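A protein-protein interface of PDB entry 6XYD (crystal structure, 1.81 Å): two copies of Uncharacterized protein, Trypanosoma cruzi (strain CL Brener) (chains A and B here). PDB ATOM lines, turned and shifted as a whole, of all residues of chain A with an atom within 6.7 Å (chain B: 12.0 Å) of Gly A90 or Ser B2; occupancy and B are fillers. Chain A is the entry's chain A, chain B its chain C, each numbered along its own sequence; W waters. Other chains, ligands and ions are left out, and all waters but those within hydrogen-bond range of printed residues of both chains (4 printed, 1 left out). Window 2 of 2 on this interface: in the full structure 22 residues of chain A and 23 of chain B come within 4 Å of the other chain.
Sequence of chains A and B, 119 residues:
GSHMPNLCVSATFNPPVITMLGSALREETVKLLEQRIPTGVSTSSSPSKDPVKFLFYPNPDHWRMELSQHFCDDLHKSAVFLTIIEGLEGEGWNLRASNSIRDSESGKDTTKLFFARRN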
ATOM      1  N   LEU A  32      12.921  -8.206  -6.879  1.00  0.00           N
ATOM      2  CA  LEU A  32      11.669  -8.212  -6.129  1.00  0.00           C
ATOM      3  C   LEU A  32      11.820  -7.383  -4.856  1.00  0.00           C
ATOM      4  O   LEU A  32      10.986  -6.513  -4.593  1.00  0.00           O
ATOM      5  CB  LEU A  32      11.244  -9.654  -5.784  1.00  0.00           C
ATOM      6  CG  LEU A  32       9.868  -9.791  -5.158  1.00  0.00           C
ATOM      7  CD1 LEU A  32       9.009 -10.728  -5.952  1.00  0.00           C
ATOM      8  CD2 LEU A  32       9.965 -10.245  -3.728  1.00  0.00           C
ATOM      9  N   ILE A  85      11.630 -10.556   4.824  1.00  0.00           N
ATOM     10  CA  ILE A  85      11.230 -11.933   5.148  1.00  0.00           C
ATOM     11  C   ILE A  85      10.109 -12.414   4.236  1.00  0.00           C
ATOM     12  O   ILE A  85      10.184 -13.518   3.689  1.00  0.00           O
ATOM     13  CB  ILE A  85      10.848 -12.042   6.661  1.00  0.00           C
ATOM     14  CG1 ILE A  85      12.098 -11.805   7.540  1.00  0.00           C
ATOM     15  CG2 ILE A  85      10.182 -13.411   6.983  1.00  0.00           C
ATOM     16  CD1 ILE A  85      11.775 -11.302   8.980  1.00  0.00           C
ATOM     17  N   GLU A  86       9.049 -11.597   4.098  1.00  0.00           N
ATOM     18  CA  GLU A  86       7.892 -11.963   3.255  1.00  0.00           C
ATOM     19  C   GLU A  86       8.283 -12.125   1.801  1.00  0.00           C
ATOM     20  O   GLU A  86       7.882 -13.102   1.156  1.00  0.00           O
ATOM     21  CB  GLU A  86       6.762 -10.942   3.398  1.00  0.00           C
ATOM     22  CG  GLU A  86       6.106 -10.960   4.773  1.00  0.00           C
ATOM     23  CD  GLU A  86       4.915 -10.035   4.920  1.00  0.00           C
ATOM     24  OE1 GLU A  86       4.962  -8.908   4.380  1.00  0.00           O
ATOM     25  OE2 GLU A  86       3.914 -10.455   5.539  1.00  0.00           O
ATOM     26  N   GLY A  87       9.100 -11.190   1.301  1.00  0.00           N
ATOM     27  CA  GLY A  87       9.574 -11.266  -0.081  1.00  0.00           C
ATOM     28  C   GLY A  87      10.385 -12.530  -0.312  1.00  0.00           C
ATOM     29  O   GLY A  87      10.166 -13.253  -1.281  1.00  0.00           O
ATOM     30  N   LEU A  88      11.289 -12.835   0.610  1.00  0.00           N
ATOM     31  CA  LEU A  88      12.124 -14.023   0.469  1.00  0.00           C
ATOM     32  C   LEU A  88      11.343 -15.309   0.588  1.00  0.00           C
ATOM     33  O   LEU A  88      11.594 -16.239  -0.184  1.00  0.00           O
ATOM     34  CB  LEU A  88      13.276 -13.996   1.461  1.00  0.00           C
ATOM     35  CG  LEU A  88      14.388 -13.002   1.112  1.00  0.00           C
ATOM     36  CD1 LEU A  88      15.320 -12.843   2.257  1.00  0.00           C
ATOM     37  CD2 LEU A  88      15.151 -13.439  -0.129  1.00  0.00           C
ATOM     38  N   GLU A  89      10.355 -15.355   1.514  1.00  0.00           N
ATOM     39  CA  GLU A  89       9.548 -16.567   1.674  1.00  0.00           C
ATOM     40  C   GLU A  89       8.843 -16.938   0.371  1.00  0.00           C
ATOM     41  O   GLU A  89       8.823 -18.115  -0.002  1.00  0.00           O
ATOM     42  CB  GLU A  89       8.545 -16.455   2.821  1.00  0.00           C
ATOM     43  CG  GLU A  89       8.044 -17.839   3.222  1.00  0.00           C
ATOM     44  CD  GLU A  89       6.914 -17.934   4.225  1.00  0.00           C
ATOM     45  OE1 GLU A  89       6.536 -16.894   4.806  1.00  0.00           O
ATOM     46  OE2 GLU A  89       6.469 -19.069   4.497  1.00  0.00           O
ATOM     47  N   GLY A  90       8.312 -15.934  -0.331  1.00  0.00           N
ATOM     48  CA  GLY A  90       7.673 -16.160  -1.624  1.00  0.00           C
ATOM     49  C   GLY A  90       8.631 -16.686  -2.686  1.00  0.00           C
ATOM     50  O   GLY A  90       8.205 -17.335  -3.636  1.00  0.00           O
ATOM     51  N   GLU A  91       9.951 -16.427  -2.511  1.00  0.00           N
ATOM     52  CA  GLU A  91      11.025 -16.860  -3.432  1.00  0.00           C
ATOM     53  C   GLU A  91      11.652 -18.206  -3.022  1.00  0.00           C
ATOM     54  O   GLU A  91      12.636 -18.646  -3.625  1.00  0.00           O
ATOM     55  CB  GLU A  91      12.106 -15.772  -3.549  1.00  0.00           C
ATOM     56  CG  GLU A  91      11.619 -14.517  -4.248  1.00  0.00           C
ATOM     57  CD  GLU A  91      11.480 -14.671  -5.747  1.00  0.00           C
ATOM     58  OE1 GLU A  91      12.510 -14.605  -6.451  1.00  0.00           O
ATOM     59  OE2 GLU A  91      10.342 -14.898  -6.215  1.00  0.00           O
ATOM     60  N   GLY A  92      11.090 -18.829  -1.999  1.00  0.00           N
ATOM     61  CA  GLY A  92      11.522 -20.145  -1.535  1.00  0.00           C
ATOM     62  C   GLY A  92      12.576 -20.144  -0.446  1.00  0.00           C
ATOM     63  O   GLY A  92      13.186 -21.191  -0.175  1.00  0.00           O
ATOM     64  N   TRP A  93      12.760 -18.991   0.227  1.00  0.00           N
ATOM     65  CA  TRP A  93      13.726 -18.873   1.322  1.00  0.00           C
ATOM     66  C   TRP A  93      12.998 -18.789   2.671  1.00  0.00           C
ATOM     67  O   TRP A  93      12.247 -17.838   2.903  1.00  0.00           O
ATOM     68  CB  TRP A  93      14.628 -17.638   1.128  1.00  0.00           C
ATOM     69  CG  TRP A  93      15.553 -17.728  -0.048  1.00  0.00           C
ATOM     70  CD1 TRP A  93      15.415 -17.090  -1.236  1.00  0.00           C
ATOM     71  CD2 TRP A  93      16.796 -18.453  -0.124  1.00  0.00           C
ATOM     72  NE1 TRP A  93      16.471 -17.388  -2.061  1.00  0.00           N
ATOM     73  CE2 TRP A  93      17.341 -18.214  -1.398  1.00  0.00           C
ATOM     74  CE3 TRP A  93      17.499 -19.290   0.762  1.00  0.00           C
ATOM     75  CZ2 TRP A  93      18.547 -18.804  -1.823  1.00  0.00           C
ATOM     76  CZ3 TRP A  93      18.701 -19.853   0.344  1.00  0.00           C
ATOM     77  CH2 TRP A  93      19.216 -19.601  -0.930  1.00  0.00           C
ATOM     78  N   GLY B   1       2.709 -12.055  -2.202  1.00  0.00           N
ATOM     79  CA  GLY B   1       1.952 -13.022  -1.422  1.00  0.00           C
ATOM     80  C   GLY B   1       1.925 -14.401  -2.050  1.00  0.00           C
ATOM     81  O   GLY B   1       0.876 -15.057  -2.058  1.00  0.00           O
ATOM     82  N   SER B   2       3.087 -14.856  -2.570  1.00  0.00           N
ATOM     83  CA  SER B   2       3.251 -16.159  -3.233  1.00  0.00           C
ATOM     84  C   SER B   2       3.067 -17.337  -2.265  1.00  0.00           C
ATOM     85  O   SER B   2       2.098 -18.091  -2.400  1.00  0.00           O
ATOM     86  CB  SER B   2       4.608 -16.235  -3.936  1.00  0.00           C
ATOM     87  OG  SER B   2       4.913 -17.539  -4.406  1.00  0.00           O
ATOM     88  N   HIS B   3       3.980 -17.468  -1.277  1.00  0.00           N
ATOM     89  CA  HIS B   3       3.956 -18.521  -0.260  1.00  0.00           C
ATOM     90  C   HIS B   3       3.978 -17.948   1.165  1.00  0.00           C
ATOM     91  O   HIS B   3       5.019 -17.495   1.634  1.00  0.00           O
ATOM     92  CB  HIS B   3       5.107 -19.539  -0.488  1.00  0.00           C
ATOM     93  CG  HIS B   3       5.304 -20.540   0.624  1.00  0.00           C
ATOM     94  ND1 HIS B   3       4.677 -21.781   0.606  1.00  0.00           N
ATOM     95  CD2 HIS B   3       6.109 -20.476   1.713  1.00  0.00           C
ATOM     96  CE1 HIS B   3       5.087 -22.405   1.701  1.00  0.00           C
ATOM     97  NE2 HIS B   3       5.949 -21.661   2.398  1.00  0.00           N
ATOM     98  N   MET B   4       2.787 -17.930   1.812  1.00  0.00           N
ATOM     99  CA  MET B   4       2.460 -17.605   3.218  1.00  0.00           C
ATOM    100  C   MET B   4       2.976 -16.219   3.835  1.00  0.00           C
ATOM    101  O   MET B   4       4.168 -15.947   3.918  1.00  0.00           O
ATOM    102  CB  MET B   4       2.863 -18.765   4.158  1.00  0.00           C
ATOM    103  CG  MET B   4       1.983 -20.023   4.034  1.00  0.00           C
ATOM    104  SD  MET B   4       0.202 -19.764   4.348  1.00  0.00           S
ATOM    105  CE  MET B   4      -0.241 -21.354   5.033  1.00  0.00           C
ATOM    106  N   PRO B   5       2.005 -15.448   4.399  1.00  0.00           N
ATOM    107  CA  PRO B   5       2.304 -14.180   5.141  1.00  0.00           C
ATOM    108  C   PRO B   5       3.183 -14.330   6.406  1.00  0.00           C
ATOM    109  O   PRO B   5       3.279 -15.418   6.960  1.00  0.00           O
ATOM    110  CB  PRO B   5       0.906 -13.732   5.583  1.00  0.00           C
ATOM    111  CG  PRO B   5       0.094 -15.044   5.578  1.00  0.00           C
ATOM    112  CD  PRO B   5       0.562 -15.721   4.382  1.00  0.00           C
ATOM    113  N   ASN B   6       3.775 -13.213   6.906  1.00  0.00           N
ATOM    114  CA  ASN B   6       4.598 -13.237   8.122  1.00  0.00           C
ATOM    115  C   ASN B   6       4.204 -12.116   9.105  1.00  0.00           C
ATOM    116  O   ASN B   6       3.529 -11.164   8.712  1.00  0.00           O
ATOM    117  CB  ASN B   6       6.087 -13.097   7.778  1.00  0.00           C
ATOM    118  CG  ASN B   6       6.672 -14.320   7.142  1.00  0.00           C
ATOM    119  OD1 ASN B   6       7.316 -15.140   7.794  1.00  0.00           O
ATOM    120  ND2 ASN B   6       6.538 -14.412   5.843  1.00  0.00           N
ATOM    121  N   LEU B   7       4.700 -12.206  10.366  1.00  0.00           N
ATOM    122  CA  LEU B   7       4.475 -11.197  11.370  1.00  0.00           C
ATOM    123  C   LEU B   7       5.779 -10.789  11.977  1.00  0.00           C
ATOM    124  O   LEU B   7       6.673 -11.617  12.141  1.00  0.00           O
ATOM    125  CB  LEU B   7       3.601 -11.730  12.539  1.00  0.00           C
ATOM    126  CG  LEU B   7       2.194 -12.198  12.293  1.00  0.00           C
ATOM    127  CD1 LEU B   7       1.516 -12.541  13.644  1.00  0.00           C
ATOM    128  CD2 LEU B   7       1.354 -11.132  11.541  1.00  0.00           C
ATOM    129  N   SER B  23       0.224  -7.598   7.661  1.00  0.00           N
ATOM    130  CA  SER B  23      -1.087  -7.352   7.056  1.00  0.00           C
ATOM    131  C   SER B  23      -2.128  -8.443   7.353  1.00  0.00           C
ATOM    132  O   SER B  23      -3.304  -8.115   7.506  1.00  0.00           O
ATOM    133  CB  SER B  23      -0.955  -7.142   5.549  1.00  0.00           C
ATOM    134  OG  SER B  23      -0.278  -8.229   4.937  1.00  0.00           O
ATOM    135  N   ALA B  24      -1.691  -9.725   7.488  1.00  0.00           N
ATOM    136  CA  ALA B  24      -2.608 -10.841   7.723  1.00  0.00           C
ATOM    137  C   ALA B  24      -2.994 -11.040   9.187  1.00  0.00           C
ATOM    138  O   ALA B  24      -3.737 -11.972   9.494  1.00  0.00           O
ATOM    139  CB  ALA B  24      -2.046 -12.119   7.130  1.00  0.00           C
ATOM    140  N   ARG B  96       9.807 -18.210  14.412  1.00  0.00           N
ATOM    141  CA  ARG B  96      10.934 -18.615  13.574  1.00  0.00           C
ATOM    142  C   ARG B  96      12.250 -18.058  14.052  1.00  0.00           C
ATOM    143  O   ARG B  96      13.272 -18.707  13.906  1.00  0.00           O
ATOM    144  CB  ARG B  96      10.687 -18.210  12.095  1.00  0.00           C
ATOM    145  CG  ARG B  96       9.571 -18.991  11.427  1.00  0.00           C
ATOM    146  CD  ARG B  96      10.085 -20.328  10.913  1.00  0.00           C
ATOM    147  NE  ARG B  96       9.119 -20.947  10.019  1.00  0.00           N
ATOM    148  CZ  ARG B  96       9.126 -20.800   8.702  1.00  0.00           C
ATOM    149  NH1 ARG B  96      10.061 -20.056   8.113  1.00  0.00           N
ATOM    150  NH2 ARG B  96       8.194 -21.379   7.962  1.00  0.00           N
ATOM    151  N   PHE B 115       7.390 -14.376  13.033  1.00  0.00           N
ATOM    152  CA  PHE B 115       6.487 -15.517  12.889  1.00  0.00           C
ATOM    153  C   PHE B 115       6.131 -15.774  11.451  1.00  0.00           C
ATOM    154  O   PHE B 115       5.996 -14.839  10.660  1.00  0.00           O
ATOM    155  CB  PHE B 115       5.166 -15.288  13.691  1.00  0.00           C
ATOM    156  CG  PHE B 115       5.383 -15.015  15.157  1.00  0.00           C
ATOM    157  CD1 PHE B 115       5.695 -13.726  15.606  1.00  0.00           C
ATOM    158  CD2 PHE B 115       5.276 -16.040  16.097  1.00  0.00           C
ATOM    159  CE1 PHE B 115       5.928 -13.465  16.972  1.00  0.00           C
ATOM    160  CE2 PHE B 115       5.516 -15.783  17.465  1.00  0.00           C
ATOM    161  CZ  PHE B 115       5.831 -14.492  17.892  1.00  0.00           C
ATOM    162  N   ALA B 116       5.921 -17.050  11.119  1.00  0.00           N
ATOM    163  CA  ALA B 116       5.466 -17.446   9.799  1.00  0.00           C
ATOM    164  C   ALA B 116       4.197 -18.262   9.971  1.00  0.00           C
ATOM    165  O   ALA B 116       3.981 -18.863  11.037  1.00  0.00           O
ATOM    166  CB  ALA B 116       6.535 -18.277   9.095  1.00  0.00           C
ATOM    167  N   ARG B 117       3.363 -18.297   8.920  1.00  0.00           N
ATOM    168  CA  ARG B 117       2.138 -19.067   8.927  1.00  0.00           C
ATOM    169  C   ARG B 117       2.464 -20.557   8.825  1.00  0.00           C
ATOM    170  O   ARG B 117       3.452 -20.940   8.196  1.00  0.00           O
ATOM    171  CB  ARG B 117       1.219 -18.599   7.782  1.00  0.00           C
ATOM    172  CG  ARG B 117      -0.243 -18.943   7.969  1.00  0.00           C
ATOM    173  CD  ARG B 117      -0.937 -18.063   8.987  1.00  0.00           C
ATOM    174  NE  ARG B 117      -2.193 -18.678   9.383  1.00  0.00           N
ATOM    175  CZ  ARG B 117      -2.828 -18.426  10.518  1.00  0.00           C
ATOM    176  NH1 ARG B 117      -2.347 -17.535  11.368  1.00  0.00           N
ATOM    177  NH2 ARG B 117      -3.961 -19.050  10.801  1.00  0.00           N
ATOM    178  N   ARG B 118       1.705 -21.358   9.589  1.00  0.00           N
ATOM    179  CA  ARG B 118       1.798 -22.812   9.698  1.00  0.00           C
ATOM    180  C   ARG B 118       1.538 -23.505   8.352  1.00  0.00           C
ATOM    181  O   ARG B 118       0.513 -23.268   7.716  1.00  0.00           O
ATOM    182  CB  ARG B 118       0.799 -23.301  10.763  1.00  0.00           C
ATOM    183  CG  ARG B 118       1.124 -24.666  11.357  1.00  0.00           C
ATOM    184  CD  ARG B 118       0.377 -24.898  12.658  1.00  0.00           C
ATOM    185  NE  ARG B 118      -1.074 -24.967  12.466  1.00  0.00           N
ATOM    186  CZ  ARG B 118      -1.967 -24.783  13.434  1.00  0.00           C
ATOM    187  NH1 ARG B 118      -1.569 -24.501  14.668  1.00  0.00           N
ATOM    188  NH2 ARG B 118      -3.264 -24.867  13.173  1.00  0.00           N
HETATM  189  O   HOH W   1       2.559  -7.437   6.018  1.00  0.00           O
HETATM  190  O   HOH W   2       8.669 -20.114   5.638  1.00  0.00           O
HETATM  191  O   HOH W   3       9.393 -16.797   6.684  1.00  0.00           O
HETATM  192  O   HOH W   4       5.021 -21.060   6.018  1.00  0.00           O
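O of Met B4 is in hydrogen-bond range of ND2 of Asn B6. The backbone carbonyl oxygen (O) of Phe B115 lies close to the side-chain amide oxygen (OD1) of Asn B6 (3.2 Å).
Among the printed residues, 7 pairs touch across the chains.
Water W4 lies within hydrogen-bond range of the backbone carbonyl oxygen (O) of Arg B117 and the side-chain carboxylate (OE2) of Glu A89. Water W2 lies within hydrogen-bond range of the guanidinium group (NH2) of Arg B96 (2.7 Å) and the side-chain carboxylate (OE2) of Glu A89 (2.7 Å). Water W1 lies within hydrogen-bond range of N of Ser B23 and OE1 of Glu A86. Water W3 bridges the side-chain amide oxygen of Asn B6 (2.9 Å) and the side-chain carboxylate of Glu A89 (3.4 Å).
Ile A85 touches Asn B6 (CG2 to OD1, 3.4 Å). CA of Gly A90 touches N of His B3, at 3.9 Å.
No position is printed for both chains. Of the 7 pairs that touch across the chains among the printed residues, none has its exchanged pair printed and touching as well.
Printed residues of chain B within 4 Å of Gly A90: Ser B2 (3.4 Å) and His B3 (3.9 Å). Ser B2 touches just one residue of chain A: Gly A90 (3.4 Å). No residue of chain B comes within 4 Å of Gly A87. Of chain B, only His B3 (3.1 Å), Met B4 (2.7 Å) and Asn B6 (2.7 Å) come within 4 Å of Glu A89. No residue of chain B comes within 4 Å of Glu A91. No residue of chain B comes within 4 Å of Gly A92. Of the printed residues of chain B, Glu A86 touches Asn B6. Printed residues of chain B within 4 Å of Ile A85: Asn B6 (3.4 Å). Printed residues of chain A within 4 Å of Met B4: Glu A89. Arg B118 touches none of the printed residues of chain A. The nearest printed residue of chain A that does not touch His B3 is Glu A86 (5.3 Å).
The backbone NH (N) of Asn B6 sits at hydrogen-bond distance from the side-chain carboxylate (OE2) of Glu A86 (3.1 Å). The side-chain carboxylate (OE2) of Glu A89 sits close to a ring nitrogen (NE2) of His B3. O of Met B4 lies close to OE1 of Glu A89, at 2.7 Å. O of Gly A90 is in hydrogen-bond range of OG of Ser B2 (3.4 Å). OE1 of Glu A89 lies within hydrogen-bond range of ND2 of Asn B6.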
